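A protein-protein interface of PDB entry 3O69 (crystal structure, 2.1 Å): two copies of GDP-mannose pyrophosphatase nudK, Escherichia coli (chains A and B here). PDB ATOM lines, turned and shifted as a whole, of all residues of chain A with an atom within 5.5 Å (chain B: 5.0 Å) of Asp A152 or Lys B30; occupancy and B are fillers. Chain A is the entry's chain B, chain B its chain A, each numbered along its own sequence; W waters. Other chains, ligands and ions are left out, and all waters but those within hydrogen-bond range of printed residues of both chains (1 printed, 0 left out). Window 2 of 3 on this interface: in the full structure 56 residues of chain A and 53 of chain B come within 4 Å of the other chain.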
ATOM      1  N   ARG A  64     -19.908  18.035  -2.599  1.00  0.00           N
ATOM      2  CA  ARG A  64     -21.179  17.492  -3.058  1.00  0.00           C
ATOM      3  C   ARG A  64     -21.241  16.038  -2.596  1.00  0.00           C
ATOM      4  O   ARG A  64     -20.315  15.254  -2.869  1.00  0.00           O
ATOM      5  CB  ARG A  64     -21.263  17.598  -4.586  1.00  0.00           C
ATOM      6  CG  ARG A  64     -22.605  17.199  -5.223  1.00  0.00           C
ATOM      7  CD  ARG A  64     -22.436  16.933  -6.747  1.00  0.00           C
ATOM      8  NE  ARG A  64     -22.638  18.122  -7.571  1.00  0.00           N
ATOM      9  CZ  ARG A  64     -21.965  18.404  -8.694  1.00  0.00           C
ATOM     10  NH1 ARG A  64     -21.004  17.592  -9.144  1.00  0.00           N
ATOM     11  NH2 ARG A  64     -22.234  19.518  -9.363  1.00  0.00           N
ATOM     12  N   GLN A  65     -22.322  15.682  -1.892  1.00  0.00           N
ATOM     13  CA  GLN A  65     -22.537  14.308  -1.429  1.00  0.00           C
ATOM     14  C   GLN A  65     -24.022  13.953  -1.397  1.00  0.00           C
ATOM     15  O   GLN A  65     -24.886  14.830  -1.433  1.00  0.00           O
ATOM     16  CB  GLN A  65     -21.905  14.078  -0.035  1.00  0.00           C
ATOM     17  CG  GLN A  65     -22.609  14.817   1.105  1.00  0.00           C
ATOM     18  CD  GLN A  65     -21.756  14.988   2.326  1.00  0.00           C
ATOM     19  OE1 GLN A  65     -21.561  14.053   3.108  1.00  0.00           O
ATOM     20  NE2 GLN A  65     -21.261  16.198   2.526  1.00  0.00           N
ATOM     21  N   PHE A  66     -24.320  12.663  -1.330  1.00  0.00           N
ATOM     22  CA  PHE A  66     -25.708  12.225  -1.144  1.00  0.00           C
ATOM     23  C   PHE A  66     -26.211  12.518   0.266  1.00  0.00           C
ATOM     24  O   PHE A  66     -25.583  12.122   1.260  1.00  0.00           O
ATOM     25  CB  PHE A  66     -25.863  10.735  -1.461  1.00  0.00           C
ATOM     26  CG  PHE A  66     -27.285  10.253  -1.416  1.00  0.00           C
ATOM     27  CD1 PHE A  66     -28.174  10.555  -2.443  1.00  0.00           C
ATOM     28  CD2 PHE A  66     -27.747   9.515  -0.333  1.00  0.00           C
ATOM     29  CE1 PHE A  66     -29.491  10.106  -2.384  1.00  0.00           C
ATOM     30  CE2 PHE A  66     -29.064   9.061  -0.288  1.00  0.00           C
ATOM     31  CZ  PHE A  66     -29.923   9.362  -1.289  1.00  0.00           C
ATOM     32  N   GLY A 146     -12.536  13.620   0.091  1.00  0.00           N
ATOM     33  CA  GLY A 146     -13.509  12.557  -0.176  1.00  0.00           C
ATOM     34  C   GLY A 146     -14.298  12.073   1.025  1.00  0.00           C
ATOM     35  O   GLY A 146     -15.196  11.245   0.893  1.00  0.00           O
ATOM     36  N   ASP A 150     -17.716   5.488   5.427  1.00  0.00           N
ATOM     37  CA  ASP A 150     -18.640   5.064   4.373  1.00  0.00           C
ATOM     38  C   ASP A 150     -19.030   6.208   3.429  1.00  0.00           C
ATOM     39  O   ASP A 150     -19.848   6.021   2.538  1.00  0.00           O
ATOM     40  CB  ASP A 150     -19.875   4.370   4.977  1.00  0.00           C
ATOM     41  CG  ASP A 150     -20.721   5.293   5.853  1.00  0.00           C
ATOM     42  OD1 ASP A 150     -20.315   6.441   6.139  1.00  0.00           O
ATOM     43  OD2 ASP A 150     -21.823   4.859   6.261  1.00  0.00           O
ATOM     44  N   GLU A 151     -18.420   7.382   3.624  1.00  0.00           N
ATOM     45  CA  GLU A 151     -18.769   8.587   2.867  1.00  0.00           C
ATOM     46  C   GLU A 151     -18.204   8.592   1.462  1.00  0.00           C
ATOM     47  O   GLU A 151     -17.107   8.099   1.220  1.00  0.00           O
ATOM     48  CB  GLU A 151     -18.304   9.856   3.600  1.00  0.00           C
ATOM     49  CG  GLU A 151     -19.040  10.105   4.886  1.00  0.00           C
ATOM     50  CD  GLU A 151     -18.521  11.308   5.660  1.00  0.00           C
ATOM     51  OE1 GLU A 151     -17.317  11.608   5.598  1.00  0.00           O
ATOM     52  OE2 GLU A 151     -19.331  11.957   6.348  1.00  0.00           O
ATOM     53  N   ASP A 152     -18.956   9.193   0.551  1.00  0.00           N
ATOM     54  CA  ASP A 152     -18.487   9.449  -0.795  1.00  0.00           C
ATOM     55  C   ASP A 152     -18.671  10.936  -1.125  1.00  0.00           C
ATOM     56  O   ASP A 152     -19.712  11.355  -1.630  1.00  0.00           O
ATOM     57  CB  ASP A 152     -19.203   8.537  -1.795  1.00  0.00           C
ATOM     58  CG  ASP A 152     -18.587   8.586  -3.181  1.00  0.00           C
ATOM     59  OD1 ASP A 152     -17.346   8.711  -3.275  1.00  0.00           O
ATOM     60  OD2 ASP A 152     -19.345   8.493  -4.178  1.00  0.00           O
ATOM     61  N   ILE A 153     -17.649  11.726  -0.830  1.00  0.00           N
ATOM     62  CA  ILE A 153     -17.718  13.175  -1.002  1.00  0.00           C
ATOM     63  C   ILE A 153     -16.960  13.605  -2.267  1.00  0.00           C
ATOM     64  O   ILE A 153     -15.784  13.248  -2.472  1.00  0.00           O
ATOM     65  CB  ILE A 153     -17.177  13.918   0.260  1.00  0.00           C
ATOM     66  CG1 ILE A 153     -17.982  13.519   1.503  1.00  0.00           C
ATOM     67  CG2 ILE A 153     -17.155  15.432   0.052  1.00  0.00           C
ATOM     68  CD1 ILE A 153     -17.557  14.214   2.829  1.00  0.00           C
ATOM     69  N   GLU A 154     -17.647  14.358  -3.116  1.00  0.00           N
ATOM     70  CA  GLU A 154     -17.021  14.950  -4.285  1.00  0.00           C
ATOM     71  C   GLU A 154     -16.591  16.391  -3.966  1.00  0.00           C
ATOM     72  O   GLU A 154     -17.377  17.171  -3.436  1.00  0.00           O
ATOM     73  CB  GLU A 154     -17.983  14.925  -5.477  1.00  0.00           C
ATOM     74  CG  GLU A 154     -17.358  15.429  -6.761  1.00  0.00           C
ATOM     75  CD  GLU A 154     -18.352  15.647  -7.884  1.00  0.00           C
ATOM     76  OE1 GLU A 154     -19.526  15.223  -7.759  1.00  0.00           O
ATOM     77  OE2 GLU A 154     -17.947  16.254  -8.903  1.00  0.00           O
ATOM     78  N   THR B   2     -21.545   8.104  -5.730  1.00  0.00           N
ATOM     79  CA  THR B   2     -22.944   8.183  -5.221  1.00  0.00           C
ATOM     80  C   THR B   2     -24.038   7.855  -6.237  1.00  0.00           C
ATOM     81  O   THR B   2     -24.986   7.134  -5.903  1.00  0.00           O
ATOM     82  CB  THR B   2     -23.269   9.569  -4.699  1.00  0.00           C
ATOM     83  OG1 THR B   2     -22.420   9.883  -3.599  1.00  0.00           O
ATOM     84  CG2 THR B   2     -24.695   9.603  -4.228  1.00  0.00           C
ATOM     85  N   LEU B  27     -25.633   2.707  -2.009  1.00  0.00           N
ATOM     86  CA  LEU B  27     -25.046   3.812  -2.733  1.00  0.00           C
ATOM     87  C   LEU B  27     -23.833   3.280  -3.494  1.00  0.00           C
ATOM     88  O   LEU B  27     -22.971   2.594  -2.915  1.00  0.00           O
ATOM     89  CB  LEU B  27     -24.642   4.919  -1.742  1.00  0.00           C
ATOM     90  CG  LEU B  27     -23.932   6.166  -2.263  1.00  0.00           C
ATOM     91  CD1 LEU B  27     -24.314   7.338  -1.416  1.00  0.00           C
ATOM     92  CD2 LEU B  27     -22.414   5.971  -2.271  1.00  0.00           C
ATOM     93  N   THR B  28     -23.786   3.597  -4.783  1.00  0.00           N
ATOM     94  CA  THR B  28     -22.647   3.249  -5.618  1.00  0.00           C
ATOM     95  C   THR B  28     -21.636   4.399  -5.686  1.00  0.00           C
ATOM     96  O   THR B  28     -21.869   5.418  -6.335  1.00  0.00           O
ATOM     97  CB  THR B  28     -23.085   2.800  -7.026  1.00  0.00           C
ATOM     98  OG1 THR B  28     -24.100   1.797  -6.901  1.00  0.00           O
ATOM     99  CG2 THR B  28     -21.891   2.227  -7.801  1.00  0.00           C
ATOM    100  N   ARG B  29     -20.521   4.217  -4.988  1.00  0.00           N
ATOM    101  CA  ARG B  29     -19.437   5.192  -4.962  1.00  0.00           C
ATOM    102  C   ARG B  29     -18.847   5.371  -6.349  1.00  0.00           C
ATOM    103  O   ARG B  29     -18.870   4.429  -7.150  1.00  0.00           O
ATOM    104  CB  ARG B  29     -18.330   4.710  -4.034  1.00  0.00           C
ATOM    105  CG  ARG B  29     -18.661   4.748  -2.569  1.00  0.00           C
ATOM    106  CD  ARG B  29     -17.355   4.625  -1.811  1.00  0.00           C
ATOM    107  NE  ARG B  29     -17.514   4.784  -0.370  1.00  0.00           N
ATOM    108  CZ  ARG B  29     -16.603   4.414   0.525  1.00  0.00           C
ATOM    109  NH1 ARG B  29     -15.461   3.852   0.143  1.00  0.00           N
ATOM    110  NH2 ARG B  29     -16.837   4.597   1.809  1.00  0.00           N
ATOM    111  N   LYS B  30     -18.314   6.567  -6.628  1.00  0.00           N
ATOM    112  CA  LYS B  30     -17.617   6.830  -7.896  1.00  0.00           C
ATOM    113  C   LYS B  30     -16.576   5.754  -8.211  1.00  0.00           C
ATOM    114  O   LYS B  30     -16.430   5.351  -9.357  1.00  0.00           O
ATOM    115  CB  LYS B  30     -16.956   8.217  -7.896  1.00  0.00           C
ATOM    116  CG  LYS B  30     -17.688   9.278  -8.718  1.00  0.00           C
ATOM    117  CD  LYS B  30     -17.491   9.097 -10.228  1.00  0.00           C
ATOM    118  CE  LYS B  30     -18.458   9.981 -11.016  1.00  0.00           C
ATOM    119  NZ  LYS B  30     -18.440   9.746 -12.493  1.00  0.00           N
ATOM    120  N   ASP B  31     -15.889   5.290  -7.167  1.00  0.00           N
ATOM    121  CA  ASP B  31     -14.794   4.317  -7.248  1.00  0.00           C
ATOM    122  C   ASP B  31     -15.177   2.930  -7.807  1.00  0.00           C
ATOM    123  O   ASP B  31     -16.310   2.688  -8.250  1.00  0.00           O
ATOM    124  CB  ASP B  31     -14.153   4.162  -5.859  1.00  0.00           C
ATOM    125  CG  ASP B  31     -13.505   5.452  -5.360  1.00  0.00           C
ATOM    126  OD1 ASP B  31     -12.379   5.781  -5.813  1.00  0.00           O
ATOM    127  OD2 ASP B  31     -14.120   6.134  -4.501  1.00  0.00           O
HETATM  128  O   HOH W   1     -19.815  10.705  -5.736  1.00  0.00           O
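The side-chain carboxylate of Asp A152 sits at hydrogen-bond distance from the backbone NH of Thr B2, 2.7 Å away.
The guanidinium group of Arg B29 sits close to the backbone carbonyl oxygen of Asp A150.
OD2 of Asp A152 lies within hydrogen-bond range of N of Lys B30 (3.3 Å).
The backbone NH of Thr B2 is in hydrogen-bond range of the backbone carbonyl oxygen of Thr B28, 2.8 Å away.
Thr B2 touches Phe A66.
CD1 of Leu B27 touches CB of Phe A66, 3.7 Å away.
Glu A151 touches Arg B29 (O to NH2, 3.6 Å).
Asp A152 touches Arg B29.
Of chain B, only Thr B2, Arg B29 and Lys B30 come within 4 Å of Asp A152.
Lys B30 touches one residue of chain A.
Of the printed residues of chain A, Thr B2 touches Phe A66 and Asp A152.
Of the printed residues of chain B, Phe A66 touches Thr B2 (3.2 Å) and Leu B27 (3.7 Å).
The nearest printed residue of chain A that does not touch Arg B29 is Gly A146 (6.9 Å).
Of the 9 printed residues of chain A, 4 touch a printed residue of chain B.
Hydrophobic or aromatic side chains of chain A within 4 Å of the printed part of chain B: Phe A66.
Among the printed residues, 7 pairs touch across the chains.
No position is printed for both chains.
Of the 7 pairs that touch across the chains among the printed residues, none has its exchanged pair printed and touching as well.
Water W1 lies within hydrogen-bond range of the side-chain carboxylate (OD2) of Asp A152 and the backbone NH (N) of Thr B2.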
